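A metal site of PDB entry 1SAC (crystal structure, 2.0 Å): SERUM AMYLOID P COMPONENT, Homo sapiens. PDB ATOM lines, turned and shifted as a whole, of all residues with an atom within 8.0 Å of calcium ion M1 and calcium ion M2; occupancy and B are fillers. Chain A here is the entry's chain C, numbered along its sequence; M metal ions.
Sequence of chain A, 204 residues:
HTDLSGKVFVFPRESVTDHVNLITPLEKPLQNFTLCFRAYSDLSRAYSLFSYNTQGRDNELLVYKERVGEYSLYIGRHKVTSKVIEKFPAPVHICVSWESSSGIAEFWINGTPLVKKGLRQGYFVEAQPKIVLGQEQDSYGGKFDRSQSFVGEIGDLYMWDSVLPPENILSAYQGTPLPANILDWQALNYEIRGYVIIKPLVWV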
ATOM      1  N   SER A  48     -26.882  22.955 -17.819  1.00  0.00           N
ATOM      2  CA  SER A  48     -26.384  23.948 -16.857  1.00  0.00           C
ATOM      3  C   SER A  48     -27.508  24.877 -16.421  1.00  0.00           C
ATOM      4  O   SER A  48     -28.185  25.440 -17.274  1.00  0.00           O
ATOM      5  CB  SER A  48     -25.257  24.759 -17.496  1.00  0.00           C
ATOM      6  OG  SER A  48     -24.853  25.833 -16.658  1.00  0.00           O
ATOM      7  N   SER A  51     -24.047  29.304 -14.378  1.00  0.00           N
ATOM      8  CA  SER A  51     -22.639  29.215 -14.797  1.00  0.00           C
ATOM      9  C   SER A  51     -21.913  30.518 -14.413  1.00  0.00           C
ATOM     10  O   SER A  51     -22.147  31.565 -15.028  1.00  0.00           O
ATOM     11  CB  SER A  51     -22.572  28.965 -16.293  1.00  0.00           C
ATOM     12  OG  SER A  51     -21.217  28.989 -16.740  1.00  0.00           O
ATOM     13  N   TYR A  52     -21.045  30.360 -13.415  1.00  0.00           N
ATOM     14  CA  TYR A  52     -20.243  31.440 -12.777  1.00  0.00           C
ATOM     15  C   TYR A  52     -18.740  31.083 -12.956  1.00  0.00           C
ATOM     16  O   TYR A  52     -18.212  30.218 -12.245  1.00  0.00           O
ATOM     17  CB  TYR A  52     -20.676  31.465 -11.293  1.00  0.00           C
ATOM     18  CG  TYR A  52     -19.972  32.475 -10.351  1.00  0.00           C
ATOM     19  CD1 TYR A  52     -18.582  32.487 -10.206  1.00  0.00           C
ATOM     20  CD2 TYR A  52     -20.751  33.382  -9.594  1.00  0.00           C
ATOM     21  CE1 TYR A  52     -17.966  33.390  -9.313  1.00  0.00           C
ATOM     22  CE2 TYR A  52     -20.148  34.267  -8.698  1.00  0.00           C
ATOM     23  CZ  TYR A  52     -18.750  34.268  -8.549  1.00  0.00           C
ATOM     24  OH  TYR A  52     -18.158  35.128  -7.678  1.00  0.00           O
ATOM     25  N   ASN A  53     -18.116  31.742 -13.927  1.00  0.00           N
ATOM     26  CA  ASN A  53     -16.680  31.531 -14.276  1.00  0.00           C
ATOM     27  C   ASN A  53     -15.888  32.819 -14.003  1.00  0.00           C
ATOM     28  O   ASN A  53     -16.423  33.932 -14.089  1.00  0.00           O
ATOM     29  CB  ASN A  53     -16.535  31.212 -15.771  1.00  0.00           C
ATOM     30  CG  ASN A  53     -16.525  29.723 -16.093  1.00  0.00           C
ATOM     31  OD1 ASN A  53     -17.174  28.939 -15.393  1.00  0.00           O
ATOM     32  ND2 ASN A  53     -15.842  29.269 -17.132  1.00  0.00           N
ATOM     33  N   ARG A  57     -10.445  30.490 -14.774  1.00  0.00           N
ATOM     34  CA  ARG A  57     -10.972  29.444 -13.900  1.00  0.00           C
ATOM     35  C   ARG A  57     -12.345  28.993 -14.363  1.00  0.00           C
ATOM     36  O   ARG A  57     -13.313  29.757 -14.305  1.00  0.00           O
ATOM     37  CB  ARG A  57     -11.054  29.954 -12.464  1.00  0.00           C
ATOM     38  CG  ARG A  57      -9.639  29.917 -11.867  1.00  0.00           C
ATOM     39  CD  ARG A  57      -9.626  30.776 -10.599  1.00  0.00           C
ATOM     40  NE  ARG A  57      -9.055  30.032  -9.458  1.00  0.00           N
ATOM     41  CZ  ARG A  57      -8.906  30.631  -8.261  1.00  0.00           C
ATOM     42  NH1 ARG A  57      -9.171  31.925  -8.124  1.00  0.00           N
ATOM     43  NH2 ARG A  57      -8.490  29.937  -7.200  1.00  0.00           N
ATOM     44  N   ASP A  58     -12.439  27.765 -14.823  1.00  0.00           N
ATOM     45  CA  ASP A  58     -13.696  27.137 -15.256  1.00  0.00           C
ATOM     46  C   ASP A  58     -14.481  26.626 -14.059  1.00  0.00           C
ATOM     47  O   ASP A  58     -13.863  26.175 -13.096  1.00  0.00           O
ATOM     48  CB  ASP A  58     -13.387  25.968 -16.201  1.00  0.00           C
ATOM     49  CG  ASP A  58     -14.662  25.556 -16.952  1.00  0.00           C
ATOM     50  OD1 ASP A  58     -15.461  26.440 -17.254  1.00  0.00           O
ATOM     51  OD2 ASP A  58     -14.792  24.351 -17.208  1.00  0.00           O
ATOM     52  N   ASN A  59     -15.796  26.687 -14.095  1.00  0.00           N
ATOM     53  CA  ASN A  59     -16.655  26.016 -13.109  1.00  0.00           C
ATOM     54  C   ASN A  59     -16.299  26.486 -11.691  1.00  0.00           C
ATOM     55  O   ASN A  59     -16.225  25.690 -10.756  1.00  0.00           O
ATOM     56  CB  ASN A  59     -16.474  24.495 -13.196  1.00  0.00           C
ATOM     57  CG  ASN A  59     -17.119  23.891 -14.438  1.00  0.00           C
ATOM     58  OD1 ASN A  59     -17.782  24.606 -15.191  1.00  0.00           O
ATOM     59  ND2 ASN A  59     -16.987  22.611 -14.704  1.00  0.00           N
ATOM     60  N   GLU A  60     -16.033  27.772 -11.601  1.00  0.00           N
ATOM     61  CA  GLU A  60     -15.789  28.398 -10.284  1.00  0.00           C
ATOM     62  C   GLU A  60     -17.006  28.249  -9.397  1.00  0.00           C
ATOM     63  O   GLU A  60     -16.933  27.873  -8.234  1.00  0.00           O
ATOM     64  CB  GLU A  60     -15.399  29.849 -10.462  1.00  0.00           C
ATOM     65  CG  GLU A  60     -14.952  30.469  -9.145  1.00  0.00           C
ATOM     66  CD  GLU A  60     -13.685  29.838  -8.594  1.00  0.00           C
ATOM     67  OE1 GLU A  60     -13.010  29.037  -9.237  1.00  0.00           O
ATOM     68  OE2 GLU A  60     -13.318  30.145  -7.444  1.00  0.00           O
ATOM     69  N   LEU A  62     -20.965  26.457 -10.331  1.00  0.00           N
ATOM     70  CA  LEU A  62     -21.815  25.893 -11.412  1.00  0.00           C
ATOM     71  C   LEU A  62     -22.934  25.058 -10.811  1.00  0.00           C
ATOM     72  O   LEU A  62     -22.641  24.120 -10.077  1.00  0.00           O
ATOM     73  CB  LEU A  62     -20.992  25.105 -12.398  1.00  0.00           C
ATOM     74  CG  LEU A  62     -21.680  24.292 -13.463  1.00  0.00           C
ATOM     75  CD1 LEU A  62     -22.569  25.104 -14.384  1.00  0.00           C
ATOM     76  CD2 LEU A  62     -20.688  23.500 -14.314  1.00  0.00           C
ATOM     77  N   TYR A  64     -25.710  22.426 -11.884  1.00  0.00           N
ATOM     78  CA  TYR A  64     -25.805  21.544 -13.067  1.00  0.00           C
ATOM     79  C   TYR A  64     -26.884  20.498 -12.804  1.00  0.00           C
ATOM     80  O   TYR A  64     -26.918  19.924 -11.706  1.00  0.00           O
ATOM     81  CB  TYR A  64     -24.478  20.895 -13.354  1.00  0.00           C
ATOM     82  CG  TYR A  64     -24.260  20.367 -14.763  1.00  0.00           C
ATOM     83  CD1 TYR A  64     -23.850  21.222 -15.791  1.00  0.00           C
ATOM     84  CD2 TYR A  64     -24.459  19.007 -15.031  1.00  0.00           C
ATOM     85  CE1 TYR A  64     -23.650  20.720 -17.080  1.00  0.00           C
ATOM     86  CE2 TYR A  64     -24.254  18.518 -16.320  1.00  0.00           C
ATOM     87  CZ  TYR A  64     -23.852  19.369 -17.344  1.00  0.00           C
ATOM     88  OH  TYR A  64     -23.645  18.886 -18.620  1.00  0.00           O
ATOM     89  N   TYR A  74     -20.797  22.665  -8.363  1.00  0.00           N
ATOM     90  CA  TYR A  74     -19.344  22.752  -8.486  1.00  0.00           C
ATOM     91  C   TYR A  74     -18.850  24.008  -7.788  1.00  0.00           C
ATOM     92  O   TYR A  74     -19.377  25.100  -8.009  1.00  0.00           O
ATOM     93  CB  TYR A  74     -18.861  22.912  -9.935  1.00  0.00           C
ATOM     94  CG  TYR A  74     -19.134  21.751 -10.887  1.00  0.00           C
ATOM     95  CD1 TYR A  74     -20.448  21.361 -11.135  1.00  0.00           C
ATOM     96  CD2 TYR A  74     -18.069  21.083 -11.526  1.00  0.00           C
ATOM     97  CE1 TYR A  74     -20.719  20.327 -12.038  1.00  0.00           C
ATOM     98  CE2 TYR A  74     -18.340  20.049 -12.428  1.00  0.00           C
ATOM     99  CZ  TYR A  74     -19.654  19.674 -12.684  1.00  0.00           C
ATOM    100  OH  TYR A  74     -19.925  18.670 -13.577  1.00  0.00           O
ATOM    101  N   ARG A  77     -14.149  23.963  -9.416  1.00  0.00           N
ATOM    102  CA  ARG A  77     -13.932  22.760 -10.236  1.00  0.00           C
ATOM    103  C   ARG A  77     -14.146  21.475  -9.432  1.00  0.00           C
ATOM    104  O   ARG A  77     -14.071  20.357  -9.982  1.00  0.00           O
ATOM    105  CB  ARG A  77     -12.509  22.760 -10.798  1.00  0.00           C
ATOM    106  CG  ARG A  77     -12.396  23.509 -12.120  1.00  0.00           C
ATOM    107  CD  ARG A  77     -11.027  24.161 -12.348  1.00  0.00           C
ATOM    108  NE  ARG A  77     -10.582  24.987 -11.229  1.00  0.00           N
ATOM    109  CZ  ARG A  77     -11.221  26.085 -10.780  1.00  0.00           C
ATOM    110  NH1 ARG A  77     -12.348  26.508 -11.363  1.00  0.00           N
ATOM    111  NH2 ARG A  77     -10.794  26.838  -9.757  1.00  0.00           N
ATOM    112  N   GLN A 135     -26.563  29.024 -21.128  1.00  0.00           N
ATOM    113  CA  GLN A 135     -25.406  28.254 -21.648  1.00  0.00           C
ATOM    114  C   GLN A 135     -24.428  27.963 -20.504  1.00  0.00           C
ATOM    115  O   GLN A 135     -24.519  28.557 -19.421  1.00  0.00           O
ATOM    116  CB  GLN A 135     -24.646  29.022 -22.725  1.00  0.00           C
ATOM    117  CG  GLN A 135     -25.489  29.375 -23.953  1.00  0.00           C
ATOM    118  CD  GLN A 135     -25.773  28.187 -24.881  1.00  0.00           C
ATOM    119  OE1 GLN A 135     -25.000  27.234 -24.917  1.00  0.00           O
ATOM    120  NE2 GLN A 135     -26.857  28.187 -25.635  1.00  0.00           N
ATOM    121  N   GLU A 136     -23.517  27.055 -20.792  1.00  0.00           N
ATOM    122  CA  GLU A 136     -22.466  26.657 -19.852  1.00  0.00           C
ATOM    123  C   GLU A 136     -21.119  27.146 -20.389  1.00  0.00           C
ATOM    124  O   GLU A 136     -20.679  26.754 -21.470  1.00  0.00           O
ATOM    125  CB  GLU A 136     -22.477  25.130 -19.702  1.00  0.00           C
ATOM    126  CG  GLU A 136     -21.917  24.659 -18.372  1.00  0.00           C
ATOM    127  CD  GLU A 136     -20.397  24.736 -18.319  1.00  0.00           C
ATOM    128  OE1 GLU A 136     -19.708  24.324 -19.324  1.00  0.00           O
ATOM    129  OE2 GLU A 136     -19.814  25.211 -17.274  1.00  0.00           O
ATOM    130  N   GLN A 137     -20.468  28.016 -19.615  1.00  0.00           N
ATOM    131  CA  GLN A 137     -19.175  28.612 -20.009  1.00  0.00           C
ATOM    132  C   GLN A 137     -18.006  27.644 -19.817  1.00  0.00           C
ATOM    133  O   GLN A 137     -17.967  26.870 -18.852  1.00  0.00           O
ATOM    134  CB  GLN A 137     -18.827  29.807 -19.121  1.00  0.00           C
ATOM    135  CG  GLN A 137     -19.830  30.947 -19.160  1.00  0.00           C
ATOM    136  CD  GLN A 137     -19.471  32.057 -18.170  1.00  0.00           C
ATOM    137  OE1 GLN A 137     -18.662  32.931 -18.491  1.00  0.00           O
ATOM    138  NE2 GLN A 137     -20.009  32.065 -16.967  1.00  0.00           N
ATOM    139  N   ASP A 138     -17.073  27.726 -20.747  1.00  0.00           N
ATOM    140  CA  ASP A 138     -15.838  26.927 -20.709  1.00  0.00           C
ATOM    141  C   ASP A 138     -14.628  27.860 -20.808  1.00  0.00           C
ATOM    142  O   ASP A 138     -13.490  27.474 -20.518  1.00  0.00           O
ATOM    143  CB  ASP A 138     -15.791  25.918 -21.852  1.00  0.00           C
ATOM    144  CG  ASP A 138     -16.275  24.534 -21.431  1.00  0.00           C
ATOM    145  OD1 ASP A 138     -16.673  24.348 -20.219  1.00  0.00           O
ATOM    146  OD2 ASP A 138     -16.290  23.578 -22.282  1.00  0.00           O
ATOM    147  N   SER A 139     -15.041  29.123 -20.905  1.00  0.00           N
ATOM    148  CA  SER A 139     -14.103  30.236 -20.818  1.00  0.00           C
ATOM    149  C   SER A 139     -14.745  31.392 -20.053  1.00  0.00           C
ATOM    150  O   SER A 139     -15.825  31.253 -19.488  1.00  0.00           O
ATOM    151  CB  SER A 139     -13.664  30.701 -22.183  1.00  0.00           C
ATOM    152  OG  SER A 139     -14.768  31.325 -22.870  1.00  0.00           O
ATOM    153  N   GLY A 142     -17.623  32.577 -22.350  1.00  0.00           N
ATOM    154  CA  GLY A 142     -17.853  31.906 -23.640  1.00  0.00           C
ATOM    155  C   GLY A 142     -17.506  30.437 -23.636  1.00  0.00           C
ATOM    156  O   GLY A 142     -17.588  29.793 -22.588  1.00  0.00           O
ATOM    157  N   LYS A 143     -17.148  29.905 -24.791  1.00  0.00           N
ATOM    158  CA  LYS A 143     -16.901  28.478 -25.018  1.00  0.00           C
ATOM    159  C   LYS A 143     -18.092  27.654 -24.551  1.00  0.00           C
ATOM    160  O   LYS A 143     -17.965  26.793 -23.683  1.00  0.00           O
ATOM    161  CB  LYS A 143     -15.653  28.023 -24.301  1.00  0.00           C
ATOM    162  CG  LYS A 143     -14.380  28.231 -25.109  1.00  0.00           C
ATOM    163  CD  LYS A 143     -13.395  27.240 -24.530  1.00  0.00           C
ATOM    164  CE  LYS A 143     -12.589  26.540 -23.445  1.00  0.00           C
ATOM    165  NZ  LYS A 143     -11.555  27.231 -22.659  1.00  0.00           N
ATOM    166  N   PHE A 144     -19.217  27.962 -25.159  1.00  0.00           N
ATOM    167  CA  PHE A 144     -20.521  27.344 -24.888  1.00  0.00           C
ATOM    168  C   PHE A 144     -20.600  25.954 -25.481  1.00  0.00           C
ATOM    169  O   PHE A 144     -19.850  25.598 -26.398  1.00  0.00           O
ATOM    170  CB  PHE A 144     -21.655  28.210 -25.407  1.00  0.00           C
ATOM    171  CG  PHE A 144     -21.624  29.636 -24.845  1.00  0.00           C
ATOM    172  CD1 PHE A 144     -21.179  29.884 -23.555  1.00  0.00           C
ATOM    173  CD2 PHE A 144     -22.040  30.702 -25.632  1.00  0.00           C
ATOM    174  CE1 PHE A 144     -21.155  31.185 -23.051  1.00  0.00           C
ATOM    175  CE2 PHE A 144     -22.022  32.005 -25.136  1.00  0.00           C
ATOM    176  CZ  PHE A 144     -21.580  32.246 -23.833  1.00  0.00           C
ATOM    177  N   ASP A 145     -21.487  25.141 -24.941  1.00  0.00           N
ATOM    178  CA  ASP A 145     -21.668  23.758 -25.402  1.00  0.00           C
ATOM    179  C   ASP A 145     -23.137  23.459 -25.606  1.00  0.00           C
ATOM    180  O   ASP A 145     -23.964  23.518 -24.704  1.00  0.00           O
ATOM    181  CB  ASP A 145     -21.069  22.778 -24.401  1.00  0.00           C
ATOM    182  CG  ASP A 145     -21.052  21.347 -24.922  1.00  0.00           C
ATOM    183  OD1 ASP A 145     -21.911  20.951 -25.723  1.00  0.00           O
ATOM    184  OD2 ASP A 145     -20.175  20.588 -24.497  1.00  0.00           O
ATOM    185  N   ARG A 146     -23.510  23.141 -26.830  1.00  0.00           N
ATOM    186  CA  ARG A 146     -24.905  22.941 -27.227  1.00  0.00           C
ATOM    187  C   ARG A 146     -25.600  21.910 -26.348  1.00  0.00           C
ATOM    188  O   ARG A 146     -26.795  22.041 -26.083  1.00  0.00           O
ATOM    189  CB  ARG A 146     -24.919  22.426 -28.687  1.00  0.00           C
ATOM    190  CG  ARG A 146     -26.313  22.576 -29.288  1.00  0.00           C
ATOM    191  CD  ARG A 146     -26.060  21.965 -30.671  1.00  0.00           C
ATOM    192  NE  ARG A 146     -27.129  22.316 -31.624  1.00  0.00           N
ATOM    193  CZ  ARG A 146     -27.601  23.494 -32.117  1.00  0.00           C
ATOM    194  NH1 ARG A 146     -26.781  24.536 -32.122  1.00  0.00           N
ATOM    195  NH2 ARG A 146     -28.840  23.531 -32.583  1.00  0.00           N
ATOM    196  N   SER A 147     -24.888  20.896 -25.891  1.00  0.00           N
ATOM    197  CA  SER A 147     -25.525  19.785 -25.161  1.00  0.00           C
ATOM    198  C   SER A 147     -25.541  20.037 -23.661  1.00  0.00           C
ATOM    199  O   SER A 147     -26.008  19.176 -22.907  1.00  0.00           O
ATOM    200  CB  SER A 147     -24.834  18.469 -25.451  1.00  0.00           C
ATOM    201  OG  SER A 147     -23.433  18.595 -25.179  1.00  0.00           O
ATOM    202  N   GLN A 148     -25.122  21.196 -23.253  1.00  0.00           N
ATOM    203  CA  GLN A 148     -25.289  21.588 -21.846  1.00  0.00           C
ATOM    204  C   GLN A 148     -26.183  22.825 -21.755  1.00  0.00           C
ATOM    205  O   GLN A 148     -26.413  23.368 -20.656  1.00  0.00           O
ATOM    206  CB  GLN A 148     -23.929  21.909 -21.228  1.00  0.00           C
ATOM    207  CG  GLN A 148     -22.944  20.743 -21.333  1.00  0.00           C
ATOM    208  CD  GLN A 148     -21.581  21.055 -20.720  1.00  0.00           C
ATOM    209  OE1 GLN A 148     -20.933  22.028 -21.103  1.00  0.00           O
ATOM    210  NE2 GLN A 148     -21.096  20.276 -19.768  1.00  0.00           N
HETATM  211 CA    CA M   1     -17.405  24.644 -17.809  1.00  0.00          CA
HETATM  212 CA    CA M   2     -18.659  22.953 -21.082  1.00  0.00          CA
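The side-chain amide nitrogen (NE2) of Gln 148 is in hydrogen-bond range of the side-chain hydroxyl (OH) of Tyr 64. O of Gln 148 sits at hydrogen-bond distance from N of Ser 48 (2.9 Å). O of Ser 51 is in hydrogen-bond range of NE2 of Gln 137, 2.9 Å away. The side-chain amide oxygen (OE1) of Gln 137 lies close to the backbone carbonyl oxygen (O) of Ser 139 (3.4 Å). The side-chain amino group (NZ) of Lys 143 is in hydrogen-bond range of the backbone carbonyl oxygen (O) of Asp 138, at 2.9 Å. The side-chain amide oxygen (OD1) of Asn 53 lies within hydrogen-bond range of the backbone NH (N) of Asn 59, 2.9 Å away. O of Asn 59 is in hydrogen-bond range of N of Arg 77, 3.0 Å away. ND2 of Asn 53 lies close to OD1 of Asp 58, 2.9 Å away.
Of the 24 residues printed, 5 come within 4 Å of calcium ion M1. The nearest printed residue that does not touch calcium ion M1 is Asn 53 (4.9 Å).
Three residues have an atom within 4 Å of calcium ion M2: Glu 136, Asp 138 and Gln 148. The nearest printed residue that does not touch calcium ion M2 is Asp 145 (4.1 Å).
Calcium ion M1 is bound by the backbone carbonyl oxygen (O) of Gln 137 (2.5 Å), the side-chain carboxylate (OE2) of Glu 136 (2.5 Å), the side-chain carboxylate (OD1) of Asp 138 (2.5 Å), the side-chain amide oxygen (OD1) of Asn 59 (2.6 Å), the side-chain carboxylate (OD2) of Asp 58 (2.7 Å), the side-chain carboxylate (OD1) of Asp 58 (2.7 Å) and the side-chain carboxylate (OE1) of Glu 136 (2.8 Å). Calcium ion M1 has seven donor atoms within binding distance.
Calcium ion M2 is bound by the side-chain amide oxygen (OE1) of Gln 148 (2.5 Å). Calcium ion M2 is bound by the side-chain carboxylate (OE1) of Glu 136 (2.5 Å). The side-chain carboxylate (OD1) of Asp 138 is bound to calcium ion M2, at 2.6 Å. The side-chain carboxylate (OD2) of Asp 138 binds calcium ion M2, 2.7 Å away.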
